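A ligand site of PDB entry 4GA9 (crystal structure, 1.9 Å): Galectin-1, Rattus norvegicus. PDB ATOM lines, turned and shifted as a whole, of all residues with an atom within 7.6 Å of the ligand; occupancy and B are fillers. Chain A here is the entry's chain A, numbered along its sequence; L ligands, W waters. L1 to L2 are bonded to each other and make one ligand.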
ATOM      1  N   SER A  29     -21.525 -24.306  -0.245  1.00  0.00           N
ATOM      2  CA  SER A  29     -21.923 -22.907  -0.301  1.00  0.00           C
ATOM      3  C   SER A  29     -22.933 -22.675   0.820  1.00  0.00           C
ATOM      4  O   SER A  29     -23.727 -23.566   1.120  1.00  0.00           O
ATOM      5  CB  SER A  29     -22.584 -22.640  -1.677  1.00  0.00           C
ATOM      6  OG  SER A  29     -23.173 -21.364  -1.781  1.00  0.00           O
ATOM      7  N   VAL A  31     -25.457 -19.178   2.658  1.00  0.00           N
ATOM      8  CA  VAL A  31     -25.904 -17.822   2.426  1.00  0.00           C
ATOM      9  C   VAL A  31     -26.565 -17.220   3.664  1.00  0.00           C
ATOM     10  O   VAL A  31     -27.356 -17.876   4.331  1.00  0.00           O
ATOM     11  CB  VAL A  31     -26.901 -17.744   1.225  1.00  0.00           C
ATOM     12  CG1 VAL A  31     -27.508 -16.344   1.086  1.00  0.00           C
ATOM     13  CG2 VAL A  31     -26.223 -18.151  -0.072  1.00  0.00           C
ATOM     14  N   ASN A  33     -28.811 -13.753   4.001  1.00  0.00           N
ATOM     15  CA  ASN A  33     -29.440 -12.626   3.319  1.00  0.00           C
ATOM     16  C   ASN A  33     -30.061 -11.666   4.318  1.00  0.00           C
ATOM     17  O   ASN A  33     -30.748 -12.096   5.242  1.00  0.00           O
ATOM     18  CB  ASN A  33     -30.532 -13.101   2.365  1.00  0.00           C
ATOM     19  CG  ASN A  33     -29.987 -13.786   1.140  1.00  0.00           C
ATOM     20  OD1 ASN A  33     -28.904 -13.456   0.649  1.00  0.00           O
ATOM     21  ND2 ASN A  33     -30.726 -14.756   0.628  1.00  0.00           N
ATOM     22  N   HIS A  44     -26.427  -9.814   0.548  1.00  0.00           N
ATOM     23  CA  HIS A  44     -26.405 -11.239   0.222  1.00  0.00           C
ATOM     24  C   HIS A  44     -24.964 -11.685   0.500  1.00  0.00           C
ATOM     25  O   HIS A  44     -24.052 -11.347  -0.250  1.00  0.00           O
ATOM     26  CB  HIS A  44     -26.803 -11.437  -1.246  1.00  0.00           C
ATOM     27  CG  HIS A  44     -26.530 -12.799  -1.789  1.00  0.00           C
ATOM     28  ND1 HIS A  44     -27.275 -13.909  -1.448  1.00  0.00           N
ATOM     29  CD2 HIS A  44     -25.621 -13.226  -2.708  1.00  0.00           C
ATOM     30  CE1 HIS A  44     -26.829 -14.960  -2.109  1.00  0.00           C
ATOM     31  NE2 HIS A  44     -25.825 -14.571  -2.881  1.00  0.00           N
ATOM     32  N   PHE A  45     -24.780 -12.409   1.604  1.00  0.00           N
ATOM     33  CA  PHE A  45     -23.457 -12.835   2.089  1.00  0.00           C
ATOM     34  C   PHE A  45     -23.308 -14.322   1.780  1.00  0.00           C
ATOM     35  O   PHE A  45     -23.981 -15.154   2.386  1.00  0.00           O
ATOM     36  CB  PHE A  45     -23.358 -12.552   3.593  1.00  0.00           C
ATOM     37  CG  PHE A  45     -22.134 -13.116   4.266  1.00  0.00           C
ATOM     38  CD1 PHE A  45     -20.904 -12.464   4.174  1.00  0.00           C
ATOM     39  CD2 PHE A  45     -22.211 -14.289   5.017  1.00  0.00           C
ATOM     40  CE1 PHE A  45     -19.782 -12.975   4.814  1.00  0.00           C
ATOM     41  CE2 PHE A  45     -21.084 -14.808   5.662  1.00  0.00           C
ATOM     42  CZ  PHE A  45     -19.863 -14.155   5.559  1.00  0.00           C
ATOM     43  N   ASN A  46     -22.450 -14.642   0.805  1.00  0.00           N
ATOM     44  CA  ASN A  46     -22.361 -15.980   0.217  1.00  0.00           C
ATOM     45  C   ASN A  46     -20.930 -16.540   0.160  1.00  0.00           C
ATOM     46  O   ASN A  46     -20.252 -16.430  -0.879  1.00  0.00           O
ATOM     47  CB  ASN A  46     -23.056 -15.966  -1.159  1.00  0.00           C
ATOM     48  CG  ASN A  46     -23.085 -17.338  -1.866  1.00  0.00           C
ATOM     49  OD1 ASN A  46     -23.245 -17.405  -3.081  1.00  0.00           O
ATOM     50  ND2 ASN A  46     -22.979 -18.427  -1.103  1.00  0.00           N
ATOM     51  N   ARG A  48     -18.536 -19.255  -0.618  1.00  0.00           N
ATOM     52  CA  ARG A  48     -18.546 -20.396  -1.540  1.00  0.00           C
ATOM     53  C   ARG A  48     -17.295 -21.240  -1.359  1.00  0.00           C
ATOM     54  O   ARG A  48     -16.181 -20.794  -1.665  1.00  0.00           O
ATOM     55  CB  ARG A  48     -18.637 -19.901  -2.985  1.00  0.00           C
ATOM     56  CG  ARG A  48     -19.870 -19.074  -3.275  1.00  0.00           C
ATOM     57  CD  ARG A  48     -19.879 -18.552  -4.708  1.00  0.00           C
ATOM     58  NE  ARG A  48     -21.105 -17.798  -4.975  1.00  0.00           N
ATOM     59  CZ  ARG A  48     -21.349 -17.117  -6.096  1.00  0.00           C
ATOM     60  NH1 ARG A  48     -20.444 -17.114  -7.073  1.00  0.00           N
ATOM     61  NH2 ARG A  48     -22.492 -16.455  -6.248  1.00  0.00           N
ATOM     62  N   ALA A  51     -18.602 -23.308  -5.485  1.00  0.00           N
ATOM     63  CA  ALA A  51     -19.891 -23.089  -6.131  1.00  0.00           C
ATOM     64  C   ALA A  51     -19.805 -21.978  -7.169  1.00  0.00           C
ATOM     65  O   ALA A  51     -19.084 -20.989  -6.975  1.00  0.00           O
ATOM     66  CB  ALA A  51     -20.953 -22.756  -5.093  1.00  0.00           C
ATOM     67  N   HIS A  52     -20.535 -22.147  -8.277  1.00  0.00           N
ATOM     68  CA  HIS A  52     -20.643 -21.127  -9.325  1.00  0.00           C
ATOM     69  C   HIS A  52     -19.300 -20.676  -9.925  1.00  0.00           C
ATOM     70  O   HIS A  52     -19.172 -19.551 -10.395  1.00  0.00           O
ATOM     71  CB  HIS A  52     -21.455 -19.909  -8.841  1.00  0.00           C
ATOM     72  CG  HIS A  52     -22.733 -20.263  -8.163  1.00  0.00           C
ATOM     73  ND1 HIS A  52     -23.876 -20.600  -8.859  1.00  0.00           N
ATOM     74  CD2 HIS A  52     -23.067 -20.311  -6.847  1.00  0.00           C
ATOM     75  CE1 HIS A  52     -24.848 -20.854  -8.000  1.00  0.00           C
ATOM     76  NE2 HIS A  52     -24.385 -20.691  -6.779  1.00  0.00           N
ATOM     77  N   GLY A  53     -18.314 -21.567  -9.899  1.00  0.00           N
ATOM     78  CA  GLY A  53     -16.988 -21.261 -10.442  1.00  0.00           C
ATOM     79  C   GLY A  53     -16.028 -20.620  -9.455  1.00  0.00           C
ATOM     80  O   GLY A  53     -14.858 -20.420  -9.769  1.00  0.00           O
ATOM     81  N   ASP A  54     -16.525 -20.299  -8.257  1.00  0.00           N
ATOM     82  CA  ASP A  54     -15.667 -19.769  -7.185  1.00  0.00           C
ATOM     83  C   ASP A  54     -15.249 -20.880  -6.233  1.00  0.00           C
ATOM     84  O   ASP A  54     -16.069 -21.736  -5.875  1.00  0.00           O
ATOM     85  CB  ASP A  54     -16.382 -18.683  -6.385  1.00  0.00           C
ATOM     86  CG  ASP A  54     -16.572 -17.394  -7.167  1.00  0.00           C
ATOM     87  OD1 ASP A  54     -15.565 -16.686  -7.432  1.00  0.00           O
ATOM     88  OD2 ASP A  54     -17.727 -17.076  -7.494  1.00  0.00           O
ATOM     89  N   VAL A  59     -18.610 -14.237  -1.663  1.00  0.00           N
ATOM     90  CA  VAL A  59     -19.225 -13.364  -2.652  1.00  0.00           C
ATOM     91  C   VAL A  59     -20.359 -12.615  -1.955  1.00  0.00           C
ATOM     92  O   VAL A  59     -21.215 -13.223  -1.298  1.00  0.00           O
ATOM     93  CB  VAL A  59     -19.794 -14.166  -3.865  1.00  0.00           C
ATOM     94  CG1 VAL A  59     -20.533 -13.262  -4.838  1.00  0.00           C
ATOM     95  CG2 VAL A  59     -18.676 -14.890  -4.593  1.00  0.00           C
ATOM     96  N   CYS A  60     -20.324 -11.290  -2.068  1.00  0.00           N
ATOM     97  CA  CYS A  60     -21.383 -10.445  -1.540  1.00  0.00           C
ATOM     98  C   CYS A  60     -22.073  -9.679  -2.660  1.00  0.00           C
ATOM     99  O   CYS A  60     -21.454  -9.289  -3.652  1.00  0.00           O
ATOM    100  CB  CYS A  60     -20.839  -9.476  -0.499  1.00  0.00           C
ATOM    101  SG  CYS A  60     -20.245 -10.270   1.009  1.00  0.00           S
ATOM    102  N   ASN A  61     -23.375  -9.484  -2.491  1.00  0.00           N
ATOM    103  CA  ASN A  61     -24.123  -8.666  -3.427  1.00  0.00           C
ATOM    104  C   ASN A  61     -25.318  -8.010  -2.762  1.00  0.00           C
ATOM    105  O   ASN A  61     -25.661  -8.310  -1.621  1.00  0.00           O
ATOM    106  CB  ASN A  61     -24.572  -9.500  -4.633  1.00  0.00           C
ATOM    107  CG  ASN A  61     -24.629  -8.691  -5.909  1.00  0.00           C
ATOM    108  OD1 ASN A  61     -24.611  -7.457  -5.879  1.00  0.00           O
ATOM    109  ND2 ASN A  61     -24.713  -9.380  -7.046  1.00  0.00           N
ATOM    110  N   SER A  62     -25.922  -7.075  -3.485  1.00  0.00           N
ATOM    111  CA  SER A  62     -27.206  -6.529  -3.136  1.00  0.00           C
ATOM    112  C   SER A  62     -28.219  -7.065  -4.137  1.00  0.00           C
ATOM    113  O   SER A  62     -27.852  -7.588  -5.205  1.00  0.00           O
ATOM    114  CB  SER A  62     -27.174  -5.007  -3.199  1.00  0.00           C
ATOM    115  OG  SER A  62     -26.685  -4.584  -4.467  1.00  0.00           O
ATOM    116  N   LYS A  63     -29.494  -6.945  -3.795  1.00  0.00           N
ATOM    117  CA  LYS A  63     -30.571  -7.340  -4.694  1.00  0.00           C
ATOM    118  C   LYS A  63     -31.668  -6.289  -4.609  1.00  0.00           C
ATOM    119  O   LYS A  63     -32.271  -6.065  -3.559  1.00  0.00           O
ATOM    120  CB  LYS A  63     -31.084  -8.734  -4.310  1.00  0.00           C
ATOM    121  CG  LYS A  63     -32.008  -9.375  -5.332  1.00  0.00           C
ATOM    122  CD  LYS A  63     -32.318 -10.809  -4.926  1.00  0.00           C
ATOM    123  CE  LYS A  63     -32.702 -11.647  -6.136  1.00  0.00           C
ATOM    124  NZ  LYS A  63     -32.947 -13.056  -5.749  1.00  0.00           N
ATOM    125  N   TRP A  68     -29.962  -8.670  -9.045  1.00  0.00           N
ATOM    126  CA  TRP A  68     -28.676  -8.678  -8.367  1.00  0.00           C
ATOM    127  C   TRP A  68     -27.882  -7.446  -8.789  1.00  0.00           C
ATOM    128  O   TRP A  68     -27.959  -7.048  -9.933  1.00  0.00           O
ATOM    129  CB  TRP A  68     -27.875  -9.929  -8.746  1.00  0.00           C
ATOM    130  CG  TRP A  68     -28.401 -11.224  -8.207  1.00  0.00           C
ATOM    131  CD1 TRP A  68     -28.818 -12.308  -8.931  1.00  0.00           C
ATOM    132  CD2 TRP A  68     -28.527 -11.584  -6.829  1.00  0.00           C
ATOM    133  NE1 TRP A  68     -29.210 -13.312  -8.077  1.00  0.00           N
ATOM    134  CE2 TRP A  68     -29.040 -12.902  -6.774  1.00  0.00           C
ATOM    135  CE3 TRP A  68     -28.271 -10.920  -5.616  1.00  0.00           C
ATOM    136  CZ2 TRP A  68     -29.296 -13.561  -5.578  1.00  0.00           C
ATOM    137  CZ3 TRP A  68     -28.533 -11.585  -4.425  1.00  0.00           C
ATOM    138  CH2 TRP A  68     -29.043 -12.887  -4.411  1.00  0.00           C
ATOM    139  N   GLY A  69     -27.123  -6.864  -7.862  1.00  0.00           N
ATOM    140  CA  GLY A  69     -26.202  -5.775  -8.209  1.00  0.00           C
ATOM    141  C   GLY A  69     -24.852  -6.321  -8.662  1.00  0.00           C
ATOM    142  O   GLY A  69     -24.764  -7.483  -9.085  1.00  0.00           O
ATOM    143  N   THR A  70     -23.799  -5.502  -8.569  1.00  0.00           N
ATOM    144  CA  THR A  70     -22.459  -5.958  -8.950  1.00  0.00           C
ATOM    145  C   THR A  70     -21.759  -6.595  -7.752  1.00  0.00           C
ATOM    146  O   THR A  70     -21.786  -6.059  -6.638  1.00  0.00           O
ATOM    147  CB  THR A  70     -21.558  -4.852  -9.574  1.00  0.00           C
ATOM    148  OG1 THR A  70     -20.903  -4.111  -8.542  1.00  0.00           O
ATOM    149  CG2 THR A  70     -22.380  -3.906 -10.419  1.00  0.00           C
ATOM    150  N   GLU A  71     -21.146  -7.747  -7.983  1.00  0.00           N
ATOM    151  CA  GLU A  71     -20.577  -8.551  -6.900  1.00  0.00           C
ATOM    152  C   GLU A  71     -19.310  -7.942  -6.298  1.00  0.00           C
ATOM    153  O   GLU A  71     -18.577  -7.196  -6.956  1.00  0.00           O
ATOM    154  CB  GLU A  71     -20.290  -9.975  -7.385  1.00  0.00           C
ATOM    155  CG  GLU A  71     -21.549 -10.763  -7.731  1.00  0.00           C
ATOM    156  CD  GLU A  71     -21.267 -12.097  -8.408  1.00  0.00           C
ATOM    157  OE1 GLU A  71     -20.160 -12.283  -8.962  1.00  0.00           O
ATOM    158  OE2 GLU A  71     -22.157 -12.957  -8.378  1.00  0.00           O
ATOM    159  N   GLN A  72     -19.089  -8.259  -5.025  1.00  0.00           N
ATOM    160  CA  GLN A  72     -17.855  -7.944  -4.322  1.00  0.00           C
ATOM    161  C   GLN A  72     -17.316  -9.269  -3.797  1.00  0.00           C
ATOM    162  O   GLN A  72     -18.077 -10.037  -3.196  1.00  0.00           O
ATOM    163  CB  GLN A  72     -18.141  -6.970  -3.182  1.00  0.00           C
ATOM    164  CG  GLN A  72     -16.928  -6.471  -2.433  1.00  0.00           C
ATOM    165  CD  GLN A  72     -17.274  -5.482  -1.342  1.00  0.00           C
ATOM    166  OE1 GLN A  72     -17.779  -4.388  -1.613  1.00  0.00           O
ATOM    167  NE2 GLN A  72     -16.994  -5.846  -0.093  1.00  0.00           N
ATOM    168  N   ARG A  73     -16.028  -9.531  -4.022  1.00  0.00           N
ATOM    169  CA  ARG A  73     -15.405 -10.749  -3.486  1.00  0.00           C
ATOM    170  C   ARG A  73     -14.355 -10.468  -2.427  1.00  0.00           C
ATOM    171  O   ARG A  73     -13.615  -9.484  -2.541  1.00  0.00           O
ATOM    172  CB  ARG A  73     -14.791 -11.580  -4.609  1.00  0.00           C
ATOM    173  CG  ARG A  73     -15.804 -12.408  -5.360  1.00  0.00           C
ATOM    174  CD  ARG A  73     -15.232 -13.014  -6.631  1.00  0.00           C
ATOM    175  NE  ARG A  73     -16.204 -13.909  -7.253  1.00  0.00           N
ATOM    176  CZ  ARG A  73     -17.270 -13.507  -7.933  1.00  0.00           C
ATOM    177  NH1 ARG A  73     -18.108 -14.405  -8.448  1.00  0.00           N
ATOM    178  NH2 ARG A  73     -17.521 -12.212  -8.107  1.00  0.00           N
ATOM    179  N   ASP A 123     -29.548 -19.800   4.049  1.00  0.00           N
ATOM    180  CA  ASP A 123     -29.740 -20.730   2.937  1.00  0.00           C
ATOM    181  C   ASP A 123     -28.447 -21.496   2.688  1.00  0.00           C
ATOM    182  O   ASP A 123     -27.383 -21.113   3.189  1.00  0.00           O
ATOM    183  CB  ASP A 123     -30.127 -19.938   1.683  1.00  0.00           C
ATOM    184  CG  ASP A 123     -30.803 -20.784   0.647  1.00  0.00           C
ATOM    185  OD1 ASP A 123     -30.489 -20.599  -0.550  1.00  0.00           O
ATOM    186  OD2 ASP A 123     -31.650 -21.631   1.005  1.00  0.00           O
HETATM  187  C1  LIG L   1     -21.656 -15.403 -12.697  1.00  0.00           C
HETATM  188  C2  LIG L   1     -21.196 -14.951 -11.314  1.00  0.00           C
HETATM  189  C3  LIG L   1     -21.917 -15.777 -10.243  1.00  0.00           C
HETATM  190  C4  LIG L   1     -23.433 -15.646 -10.390  1.00  0.00           C
HETATM  191  C5  LIG L   1     -23.863 -15.919 -11.846  1.00  0.00           C
HETATM  192  C6  LIG L   1     -25.285 -15.456 -12.090  1.00  0.00           C
HETATM  193  O1  LIG L   1     -21.287 -16.750 -12.914  1.00  0.00           O
HETATM  194  O2  LIG L   1     -19.807 -15.097 -11.225  1.00  0.00           O
HETATM  195  O3  LIG L   1     -21.504 -15.365  -8.950  1.00  0.00           O
HETATM  196  O4  LIG L   1     -24.048 -16.536  -9.480  1.00  0.00           O
HETATM  197  O5  LIG L   1     -23.056 -15.256 -12.796  1.00  0.00           O
HETATM  198  O6  LIG L   1     -26.160 -16.542 -11.868  1.00  0.00           O
HETATM  199  C1  LG2 L   2     -25.108 -16.055  -8.673  1.00  0.00           C
HETATM  200  C2  LG2 L   2     -25.716 -17.196  -7.864  1.00  0.00           C
HETATM  201  C3  LG2 L   2     -26.756 -16.663  -6.881  1.00  0.00           C
HETATM  202  C4  LG2 L   2     -26.175 -15.514  -6.050  1.00  0.00           C
HETATM  203  C5  LG2 L   2     -25.619 -14.467  -7.009  1.00  0.00           C
HETATM  204  C6  LG2 L   2     -25.038 -13.277  -6.263  1.00  0.00           C
HETATM  205  O1  LG2 L   2     -26.337 -18.112  -8.743  1.00  0.00           O
HETATM  206  O2  LG2 L   2     -27.219 -17.683  -6.028  1.00  0.00           O
HETATM  207  O3  LG2 L   2     -25.176 -16.000  -5.165  1.00  0.00           O
HETATM  208  O4  LG2 L   2     -24.620 -15.035  -7.818  1.00  0.00           O
HETATM  209  O5  LG2 L   2     -24.461 -12.377  -7.184  1.00  0.00           O
HETATM  210  O   HOH W   1     -25.365 -18.675  -4.091  1.00  0.00           O
HETATM  211  O   HOH W   2     -29.695 -16.995  -5.097  1.00  0.00           O
HETATM  212  O   HOH W   3     -20.974 -16.052 -16.022  1.00  0.00           O
HETATM  213  O   HOH W   4     -18.443 -17.056 -10.331  1.00  0.00           O
HETATM  214  O   HOH W   5     -25.218 -12.187 -10.068  1.00  0.00           O
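The side-chain carboxylate (OE2) of Glu 71 is in hydrogen-bond range of an oxygen (O3) of LIG L1, at 2.6 Å. An oxygen (O3) of LG2 L2 lies within hydrogen-bond range of the side-chain amide oxygen (OD1) of Asn 46. O5 of LG2 L2 is in hydrogen-bond range of ND2 of Asn 61. NH1 of Arg 48 is in hydrogen-bond range of O3 of LIG L1. An oxygen (O2) of LIG L1 sits at hydrogen-bond distance from the guanidinium group of Arg 73 (3.3 Å). A ring nitrogen (NE2) of His 44 is in hydrogen-bond range of an oxygen (O3) of LG2 L2 (2.8 Å).
CE1 of His 52 touches O1 of LG2 L2 (3.2 Å). CZ2 of Trp 68 touches C4 of LG2 L2, 3.7 Å away. Hydrophobic or aromatic side chains within 4 Å of the ligand: His 44, His 52 and Trp 68. Along chain A the residues within 4 Å of the ligand span positions 44 to 73.
The side-chain hydroxyl (OG) of Ser 29 sits at hydrogen-bond distance from the side-chain amide nitrogen (ND2) of Asn 46, 3.0 Å away. NE of Arg 48 is in hydrogen-bond range of OD1 of Asn 46, 2.9 Å away. OE1 of Glu 71 is in salt-bridge range of NH2 of Arg 73. The guanidinium group of Arg 48 lies within salt-bridge range of the side-chain carboxylate of Asp 54, at 2.7 Å. A ring nitrogen (ND1) of His 44 sits at hydrogen-bond distance from the side-chain amide oxygen of Asn 33, 2.7 Å away. The side-chain amide oxygen (OD1) of Asn 61 lies close to the backbone carbonyl oxygen (O) of Thr 70, at 3.2 Å. The backbone NH (N) of His 44 lies within hydrogen-bond range of the backbone carbonyl oxygen (O) of Asn 61 (2.7 Å). The backbone carbonyl oxygen (O) of Val 59 lies within hydrogen-bond range of the backbone NH (N) of Asn 46, 2.8 Å away.
Water W4 lies within hydrogen-bond range of an oxygen (O2) of LIG L1, the backbone carbonyl oxygen (O) of His 52, the side-chain carboxylate (OD2) of Asp 54 and the guanidinium group (NH1) of Arg 73. Water W1 bridges OD1 of Asn 46 (2.7 Å) and O2 of LG2 L2 (2.9 Å).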
